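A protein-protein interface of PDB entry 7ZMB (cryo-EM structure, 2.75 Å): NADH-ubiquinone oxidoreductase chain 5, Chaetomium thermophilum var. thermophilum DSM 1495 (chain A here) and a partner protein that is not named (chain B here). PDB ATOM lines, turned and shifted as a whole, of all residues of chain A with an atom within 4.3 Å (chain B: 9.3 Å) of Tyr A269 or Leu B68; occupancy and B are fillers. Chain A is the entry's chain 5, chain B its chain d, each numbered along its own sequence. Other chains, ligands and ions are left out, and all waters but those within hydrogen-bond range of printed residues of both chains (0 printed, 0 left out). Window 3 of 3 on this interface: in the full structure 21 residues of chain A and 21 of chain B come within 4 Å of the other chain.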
ATOM      1  N   SER A 199      -5.867 -12.813 -17.314  1.00  0.00           N
ATOM      2  CA  SER A 199      -4.983 -13.336 -18.343  1.00  0.00           C
ATOM      3  C   SER A 199      -4.879 -14.850 -18.252  1.00  0.00           C
ATOM      4  O   SER A 199      -4.843 -15.542 -19.275  1.00  0.00           O
ATOM      5  CB  SER A 199      -3.611 -12.690 -18.209  1.00  0.00           C
ATOM      6  OG  SER A 199      -3.181 -12.765 -16.866  1.00  0.00           O
ATOM      7  N   ALA A 201      -7.119 -16.870 -16.505  1.00  0.00           N
ATOM      8  CA  ALA A 201      -8.406 -17.549 -16.356  1.00  0.00           C
ATOM      9  C   ALA A 201      -8.767 -18.468 -17.519  1.00  0.00           C
ATOM     10  O   ALA A 201      -9.288 -19.565 -17.256  1.00  0.00           O
ATOM     11  CB  ALA A 201      -9.514 -16.515 -16.127  1.00  0.00           C
ATOM     12  N   PRO A 202      -8.541 -18.112 -18.793  1.00  0.00           N
ATOM     13  CA  PRO A 202      -8.891 -19.032 -19.885  1.00  0.00           C
ATOM     14  C   PRO A 202      -8.125 -20.343 -19.901  1.00  0.00           C
ATOM     15  O   PRO A 202      -8.324 -21.153 -20.808  1.00  0.00           O
ATOM     16  CB  PRO A 202      -8.568 -18.211 -21.136  1.00  0.00           C
ATOM     17  CG  PRO A 202      -7.639 -17.196 -20.681  1.00  0.00           C
ATOM     18  CD  PRO A 202      -8.088 -16.824 -19.332  1.00  0.00           C
ATOM     19  N   TYR A 203      -7.244 -20.570 -18.932  1.00  0.00           N
ATOM     20  CA  TYR A 203      -6.467 -21.795 -18.902  1.00  0.00           C
ATOM     21  C   TYR A 203      -6.600 -22.574 -17.610  1.00  0.00           C
ATOM     22  O   TYR A 203      -6.163 -23.726 -17.562  1.00  0.00           O
ATOM     23  CB  TYR A 203      -4.987 -21.491 -19.147  1.00  0.00           C
ATOM     24  CG  TYR A 203      -4.766 -20.496 -20.245  1.00  0.00           C
ATOM     25  CD1 TYR A 203      -4.669 -20.903 -21.561  1.00  0.00           C
ATOM     26  CD2 TYR A 203      -4.673 -19.145 -19.969  1.00  0.00           C
ATOM     27  CE1 TYR A 203      -4.474 -19.998 -22.566  1.00  0.00           C
ATOM     28  CE2 TYR A 203      -4.479 -18.238 -20.971  1.00  0.00           C
ATOM     29  CZ  TYR A 203      -4.375 -18.665 -22.268  1.00  0.00           C
ATOM     30  OH  TYR A 203      -4.174 -17.750 -23.273  1.00  0.00           O
ATOM     31  N   VAL A 209     -12.951 -22.613 -11.536  1.00  0.00           N
ATOM     32  CA  VAL A 209     -13.765 -21.482 -11.961  1.00  0.00           C
ATOM     33  C   VAL A 209     -15.105 -21.484 -11.237  1.00  0.00           C
ATOM     34  O   VAL A 209     -15.561 -20.441 -10.759  1.00  0.00           O
ATOM     35  CB  VAL A 209     -13.941 -21.476 -13.489  1.00  0.00           C
ATOM     36  CG1 VAL A 209     -14.562 -20.164 -13.948  1.00  0.00           C
ATOM     37  CG2 VAL A 209     -12.612 -21.678 -14.172  1.00  0.00           C
ATOM     38  N   PRO A 265     -14.162 -11.408 -17.077  1.00  0.00           N
ATOM     39  CA  PRO A 265     -13.113 -12.203 -17.728  1.00  0.00           C
ATOM     40  C   PRO A 265     -12.867 -13.529 -17.045  1.00  0.00           C
ATOM     41  O   PRO A 265     -12.438 -14.488 -17.696  1.00  0.00           O
ATOM     42  CB  PRO A 265     -11.884 -11.293 -17.644  1.00  0.00           C
ATOM     43  CG  PRO A 265     -12.426  -9.948 -17.558  1.00  0.00           C
ATOM     44  CD  PRO A 265     -13.655 -10.072 -16.722  1.00  0.00           C
ATOM     45  N   LEU A 266     -13.122 -13.610 -15.743  1.00  0.00           N
ATOM     46  CA  LEU A 266     -12.934 -14.840 -14.990  1.00  0.00           C
ATOM     47  C   LEU A 266     -14.165 -15.740 -15.049  1.00  0.00           C
ATOM     48  O   LEU A 266     -14.048 -16.930 -15.351  1.00  0.00           O
ATOM     49  CB  LEU A 266     -12.575 -14.493 -13.540  1.00  0.00           C
ATOM     50  CG  LEU A 266     -12.504 -15.585 -12.473  1.00  0.00           C
ATOM     51  CD1 LEU A 266     -11.656 -16.758 -12.938  1.00  0.00           C
ATOM     52  CD2 LEU A 266     -11.954 -14.996 -11.187  1.00  0.00           C
ATOM     53  N   ILE A 267     -15.352 -15.186 -14.786  1.00  0.00           N
ATOM     54  CA  ILE A 267     -16.540 -16.021 -14.656  1.00  0.00           C
ATOM     55  C   ILE A 267     -17.062 -16.484 -16.005  1.00  0.00           C
ATOM     56  O   ILE A 267     -17.876 -17.412 -16.063  1.00  0.00           O
ATOM     57  CB  ILE A 267     -17.653 -15.284 -13.891  1.00  0.00           C
ATOM     58  CG1 ILE A 267     -18.098 -14.034 -14.646  1.00  0.00           C
ATOM     59  CG2 ILE A 267     -17.166 -14.891 -12.514  1.00  0.00           C
ATOM     60  CD1 ILE A 267     -19.345 -13.382 -14.074  1.00  0.00           C
ATOM     61  N   GLU A 268     -16.609 -15.872 -17.100  1.00  0.00           N
ATOM     62  CA  GLU A 268     -17.112 -16.237 -18.415  1.00  0.00           C
ATOM     63  C   GLU A 268     -16.671 -17.621 -18.867  1.00  0.00           C
ATOM     64  O   GLU A 268     -17.213 -18.127 -19.853  1.00  0.00           O
ATOM     65  CB  GLU A 268     -16.680 -15.207 -19.459  1.00  0.00           C
ATOM     66  CG  GLU A 268     -17.703 -14.112 -19.703  1.00  0.00           C
ATOM     67  CD  GLU A 268     -19.049 -14.655 -20.136  1.00  0.00           C
ATOM     68  OE1 GLU A 268     -19.102 -15.783 -20.666  1.00  0.00           O
ATOM     69  OE2 GLU A 268     -20.060 -13.953 -19.941  1.00  0.00           O
ATOM     70  N   TYR A 269     -15.709 -18.241 -18.185  1.00  0.00           N
ATOM     71  CA  TYR A 269     -15.227 -19.562 -18.558  1.00  0.00           C
ATOM     72  C   TYR A 269     -15.890 -20.666 -17.752  1.00  0.00           C
ATOM     73  O   TYR A 269     -15.291 -21.725 -17.541  1.00  0.00           O
ATOM     74  CB  TYR A 269     -13.710 -19.637 -18.420  1.00  0.00           C
ATOM     75  CG  TYR A 269     -12.991 -18.750 -19.396  1.00  0.00           C
ATOM     76  CD1 TYR A 269     -12.950 -19.064 -20.745  1.00  0.00           C
ATOM     77  CD2 TYR A 269     -12.354 -17.596 -18.973  1.00  0.00           C
ATOM     78  CE1 TYR A 269     -12.296 -18.252 -21.645  1.00  0.00           C
ATOM     79  CE2 TYR A 269     -11.698 -16.777 -19.864  1.00  0.00           C
ATOM     80  CZ  TYR A 269     -11.676 -17.108 -21.199  1.00  0.00           C
ATOM     81  OH  TYR A 269     -11.017 -16.294 -22.091  1.00  0.00           O
ATOM     82  N   SER A 270     -17.118 -20.441 -17.301  1.00  0.00           N
ATOM     83  CA  SER A 270     -17.905 -21.501 -16.677  1.00  0.00           C
ATOM     84  C   SER A 270     -19.369 -21.107 -16.784  1.00  0.00           C
ATOM     85  O   SER A 270     -19.804 -20.163 -16.118  1.00  0.00           O
ATOM     86  CB  SER A 270     -17.494 -21.711 -15.227  1.00  0.00           C
ATOM     87  OG  SER A 270     -17.945 -20.643 -14.417  1.00  0.00           O
ATOM     88  N   PHE A 506     -15.352  -8.672 -20.484  1.00  0.00           N
ATOM     89  CA  PHE A 506     -15.043  -9.724 -21.441  1.00  0.00           C
ATOM     90  C   PHE A 506     -16.303 -10.511 -21.766  1.00  0.00           C
ATOM     91  O   PHE A 506     -17.014 -10.959 -20.862  1.00  0.00           O
ATOM     92  CB  PHE A 506     -13.960 -10.661 -20.903  1.00  0.00           C
ATOM     93  CG  PHE A 506     -13.504 -11.681 -21.899  1.00  0.00           C
ATOM     94  CD1 PHE A 506     -12.516 -11.377 -22.816  1.00  0.00           C
ATOM     95  CD2 PHE A 506     -14.069 -12.944 -21.926  1.00  0.00           C
ATOM     96  CE1 PHE A 506     -12.095 -12.310 -23.736  1.00  0.00           C
ATOM     97  CE2 PHE A 506     -13.654 -13.882 -22.844  1.00  0.00           C
ATOM     98  CZ  PHE A 506     -12.664 -13.565 -23.749  1.00  0.00           C
ATOM     99  N   HIS A 508     -17.705 -13.720 -24.402  1.00  0.00           N
ATOM    100  CA  HIS A 508     -17.170 -14.811 -25.254  1.00  0.00           C
ATOM    101  C   HIS A 508     -18.080 -15.041 -26.475  1.00  0.00           C
ATOM    102  O   HIS A 508     -19.301 -15.160 -26.270  1.00  0.00           O
ATOM    103  CB  HIS A 508     -16.859 -16.078 -24.448  1.00  0.00           C
ATOM    104  CG  HIS A 508     -15.758 -16.876 -25.061  1.00  0.00           C
ATOM    105  ND1 HIS A 508     -15.999 -17.922 -25.929  1.00  0.00           N
ATOM    106  CD2 HIS A 508     -14.417 -16.761 -24.971  1.00  0.00           C
ATOM    107  CE1 HIS A 508     -14.853 -18.429 -26.332  1.00  0.00           C
ATOM    108  NE2 HIS A 508     -13.867 -17.735 -25.757  1.00  0.00           N
ATOM    109  N   CYS B  59       1.419  -6.022 -20.159  1.00  0.00           N
ATOM    110  CA  CYS B  59       0.755  -6.361 -21.415  1.00  0.00           C
ATOM    111  C   CYS B  59      -0.759  -6.343 -21.280  1.00  0.00           C
ATOM    112  O   CYS B  59      -1.457  -5.868 -22.180  1.00  0.00           O
ATOM    113  CB  CYS B  59       1.200  -7.727 -21.929  1.00  0.00           C
ATOM    114  SG  CYS B  59       2.892  -7.901 -22.475  1.00  0.00           S
ATOM    115  N   TYR B  60      -1.285  -6.875 -20.176  1.00  0.00           N
ATOM    116  CA  TYR B  60      -2.726  -7.045 -20.062  1.00  0.00           C
ATOM    117  C   TYR B  60      -3.467  -5.729 -20.232  1.00  0.00           C
ATOM    118  O   TYR B  60      -4.553  -5.691 -20.822  1.00  0.00           O
ATOM    119  CB  TYR B  60      -3.097  -7.668 -18.723  1.00  0.00           C
ATOM    120  CG  TYR B  60      -4.578  -7.887 -18.651  1.00  0.00           C
ATOM    121  CD1 TYR B  60      -5.183  -8.822 -19.464  1.00  0.00           C
ATOM    122  CD2 TYR B  60      -5.381  -7.118 -17.819  1.00  0.00           C
ATOM    123  CE1 TYR B  60      -6.532  -9.019 -19.430  1.00  0.00           C
ATOM    124  CE2 TYR B  60      -6.738  -7.313 -17.776  1.00  0.00           C
ATOM    125  CZ  TYR B  60      -7.307  -8.269 -18.590  1.00  0.00           C
ATOM    126  OH  TYR B  60      -8.657  -8.492 -18.573  1.00  0.00           O
ATOM    127  N   GLU B  63      -2.816  -4.379 -24.154  1.00  0.00           N
ATOM    128  CA  GLU B  63      -3.491  -5.051 -25.254  1.00  0.00           C
ATOM    129  C   GLU B  63      -4.997  -5.127 -25.068  1.00  0.00           C
ATOM    130  O   GLU B  63      -5.749  -4.754 -25.973  1.00  0.00           O
ATOM    131  CB  GLU B  63      -2.911  -6.458 -25.446  1.00  0.00           C
ATOM    132  CG  GLU B  63      -1.484  -6.460 -25.970  1.00  0.00           C
ATOM    133  CD  GLU B  63      -1.221  -5.346 -26.969  1.00  0.00           C
ATOM    134  OE1 GLU B  63      -1.985  -5.216 -27.949  1.00  0.00           O
ATOM    135  OE2 GLU B  63      -0.247  -4.590 -26.769  1.00  0.00           O
ATOM    136  N   GLY B  64      -5.464  -5.606 -23.923  1.00  0.00           N
ATOM    137  CA  GLY B  64      -6.884  -5.600 -23.653  1.00  0.00           C
ATOM    138  C   GLY B  64      -7.644  -6.687 -24.380  1.00  0.00           C
ATOM    139  O   GLY B  64      -7.566  -7.864 -24.016  1.00  0.00           O
ATOM    140  N   VAL B  65      -8.399  -6.294 -25.408  1.00  0.00           N
ATOM    141  CA  VAL B  65      -9.154  -7.263 -26.198  1.00  0.00           C
ATOM    142  C   VAL B  65      -8.220  -8.296 -26.812  1.00  0.00           C
ATOM    143  O   VAL B  65      -8.448  -9.507 -26.704  1.00  0.00           O
ATOM    144  CB  VAL B  65      -9.985  -6.540 -27.270  1.00  0.00           C
ATOM    145  CG1 VAL B  65     -10.396  -7.498 -28.355  1.00  0.00           C
ATOM    146  CG2 VAL B  65     -11.220  -5.954 -26.640  1.00  0.00           C
ATOM    147  N   ASN B  66      -7.157  -7.840 -27.462  1.00  0.00           N
ATOM    148  CA  ASN B  66      -6.182  -8.753 -28.053  1.00  0.00           C
ATOM    149  C   ASN B  66      -5.018  -9.055 -27.108  1.00  0.00           C
ATOM    150  O   ASN B  66      -3.850  -9.026 -27.487  1.00  0.00           O
ATOM    151  CB  ASN B  66      -5.709  -8.190 -29.392  1.00  0.00           C
ATOM    152  CG  ASN B  66      -4.864  -6.930 -29.251  1.00  0.00           C
ATOM    153  OD1 ASN B  66      -4.567  -6.471 -28.149  1.00  0.00           O
ATOM    154  ND2 ASN B  66      -4.475  -6.360 -30.386  1.00  0.00           N
ATOM    155  N   HIS B  67      -5.341  -9.433 -25.869  1.00  0.00           N
ATOM    156  CA  HIS B  67      -4.303  -9.785 -24.864  1.00  0.00           C
ATOM    157  C   HIS B  67      -4.051 -11.291 -24.881  1.00  0.00           C
ATOM    158  O   HIS B  67      -2.964 -11.710 -24.462  1.00  0.00           O
ATOM    159  CB  HIS B  67      -4.733  -9.326 -23.468  1.00  0.00           C
ATOM    160  CG  HIS B  67      -5.621 -10.279 -22.738  1.00  0.00           C
ATOM    161  ND1 HIS B  67      -5.135 -11.176 -21.809  1.00  0.00           N
ATOM    162  CD2 HIS B  67      -6.955 -10.468 -22.778  1.00  0.00           C
ATOM    163  CE1 HIS B  67      -6.133 -11.876 -21.313  1.00  0.00           C
ATOM    164  NE2 HIS B  67      -7.259 -11.459 -21.889  1.00  0.00           N
ATOM    165  N   LEU B  68      -5.026 -12.064 -25.358  1.00  0.00           N
ATOM    166  CA  LEU B  68      -4.874 -13.507 -25.354  1.00  0.00           C
ATOM    167  C   LEU B  68      -4.000 -14.004 -26.490  1.00  0.00           C
ATOM    168  O   LEU B  68      -3.725 -15.206 -26.556  1.00  0.00           O
ATOM    169  CB  LEU B  68      -6.250 -14.166 -25.407  1.00  0.00           C
ATOM    170  CG  LEU B  68      -7.065 -13.971 -24.132  1.00  0.00           C
ATOM    171  CD1 LEU B  68      -8.517 -14.349 -24.341  1.00  0.00           C
ATOM    172  CD2 LEU B  68      -6.459 -14.790 -23.007  1.00  0.00           C
ATOM    173  N   GLU B  69      -3.543 -13.115 -27.375  1.00  0.00           N
ATOM    174  CA  GLU B  69      -2.740 -13.544 -28.509  1.00  0.00           C
ATOM    175  C   GLU B  69      -1.521 -12.664 -28.761  1.00  0.00           C
ATOM    176  O   GLU B  69      -0.925 -12.762 -29.840  1.00  0.00           O
ATOM    177  CB  GLU B  69      -3.600 -13.604 -29.778  1.00  0.00           C
ATOM    178  CG  GLU B  69      -4.034 -12.251 -30.308  1.00  0.00           C
ATOM    179  CD  GLU B  69      -4.394 -12.296 -31.781  1.00  0.00           C
ATOM    180  OE1 GLU B  69      -3.985 -13.259 -32.464  1.00  0.00           O
ATOM    181  OE2 GLU B  69      -5.086 -11.372 -32.256  1.00  0.00           O
ATOM    182  N   LYS B  70      -1.121 -11.823 -27.816  1.00  0.00           N
ATOM    183  CA  LYS B  70       0.066 -10.999 -28.014  1.00  0.00           C
ATOM    184  C   LYS B  70       1.099 -11.145 -26.908  1.00  0.00           C
ATOM    185  O   LYS B  70       2.298 -11.143 -27.191  1.00  0.00           O
ATOM    186  CB  LYS B  70      -0.336  -9.527 -28.162  1.00  0.00           C
ATOM    187  CG  LYS B  70      -0.885  -9.197 -29.541  1.00  0.00           C
ATOM    188  CD  LYS B  70      -1.172  -7.717 -29.691  1.00  0.00           C
ATOM    189  CE  LYS B  70       0.110  -6.918 -29.841  1.00  0.00           C
ATOM    190  NZ  LYS B  70      -0.165  -5.460 -29.968  1.00  0.00           N
ATOM    191  N   CYS B  71       0.669 -11.274 -25.655  1.00  0.00           N
ATOM    192  CA  CYS B  71       1.579 -11.611 -24.567  1.00  0.00           C
ATOM    193  C   CYS B  71       1.117 -12.857 -23.828  1.00  0.00           C
ATOM    194  O   CYS B  71       0.906 -12.824 -22.613  1.00  0.00           O
ATOM    195  CB  CYS B  71       1.746 -10.453 -23.576  1.00  0.00           C
ATOM    196  SG  CYS B  71       2.619  -8.981 -24.176  1.00  0.00           S
ATOM    197  N   GLY B  72       0.925 -13.952 -24.557  1.00  0.00           N
ATOM    198  CA  GLY B  72       0.748 -15.246 -23.930  1.00  0.00           C
ATOM    199  C   GLY B  72       2.069 -15.923 -23.642  1.00  0.00           C
ATOM    200  O   GLY B  72       2.132 -16.877 -22.865  1.00  0.00           O
ATOM    201  N   LYS B  73       3.139 -15.446 -24.281  1.00  0.00           N
ATOM    202  CA  LYS B  73       4.461 -16.008 -24.024  1.00  0.00           C
ATOM    203  C   LYS B  73       4.915 -15.699 -22.606  1.00  0.00           C
ATOM    204  O   LYS B  73       5.428 -16.577 -21.902  1.00  0.00           O
ATOM    205  CB  LYS B  73       5.467 -15.474 -25.041  1.00  0.00           C
ATOM    206  CG  LYS B  73       6.902 -15.871 -24.749  1.00  0.00           C
ATOM    207  CD  LYS B  73       7.831 -15.452 -25.873  1.00  0.00           C
ATOM    208  CE  LYS B  73       9.284 -15.611 -25.468  1.00  0.00           C
ATOM    209  NZ  LYS B  73       9.645 -14.695 -24.352  1.00  0.00           N
ATOM    210  N   ARG B  75       2.826 -15.393 -20.284  1.00  0.00           N
ATOM    211  CA  ARG B  75       1.819 -16.079 -19.436  1.00  0.00           C
ATOM    212  C   ARG B  75       2.303 -17.477 -19.074  1.00  0.00           C
ATOM    213  O   ARG B  75       2.152 -17.874 -17.911  1.00  0.00           O
ATOM    214  CB  ARG B  75       0.504 -16.157 -20.210  1.00  0.00           C
ATOM    215  CG  ARG B  75      -0.730 -16.288 -19.338  1.00  0.00           C
ATOM    216  CD  ARG B  75      -1.947 -16.356 -20.226  1.00  0.00           C
ATOM    217  NE  ARG B  75      -2.315 -15.092 -20.840  1.00  0.00           N
ATOM    218  CZ  ARG B  75      -2.459 -14.902 -22.146  1.00  0.00           C
ATOM    219  NH1 ARG B  75      -2.803 -13.714 -22.605  1.00  0.00           N
ATOM    220  NH2 ARG B  75      -2.264 -15.900 -22.988  1.00  0.00           N
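Among the printed residues, merely in contact across the chains: Ser A199 with His B67, Pro A202 with Leu B68, Tyr A203 with Leu B68 and Tyr A269 with Leu B68.
Of chain B, only Leu B68 comes within 4 Å of Tyr A269. Of chain A, only Pro A202 (3.5 Å), Tyr A203 (3.7 Å) and Tyr A269 (3.9 Å) come within 4 Å of Leu B68. Pro A202 touches one residue of chain B. Printed residues of chain A within 4 Å of His B67: Ser A199. Of the printed residues of chain B, Tyr A203 touches Leu B68 and Arg B75. Glu B63 touches none of the printed residues of chain A. Ile A267 touches none of the printed residues of chain B. The nearest residue of chain B that does not touch Tyr A269 is His B67 (6.1 Å). The nearest printed residue of chain A that does not touch Leu B68 is Ser A199 (4.1 Å). The nearest printed residue of chain A that does not touch His B67 is Phe A506 (5.2 Å).
NH1 of Arg B75 lies within hydrogen-bond range of O of His B67 (2.7 Å). SG of Cys B71 is disulfide-bonded to SG of Cys B59 (2.0 Å).
Hydrophobic or aromatic side chains of chain A that line the printed part of chain B: Pro A202, Tyr A203 and Tyr A269. Among the printed residues, no Asp or Glu carboxylate lies within 4 Å of a Lys or Arg side-chain nitrogen of the other chain.
NE of Arg B75 lies within hydrogen-bond range of O of Ser A199, 3.0 Å away. The guanidinium group (NH2) of Arg B75 lies within hydrogen-bond range of the side-chain hydroxyl (OH) of Tyr A203 (2.7 Å).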
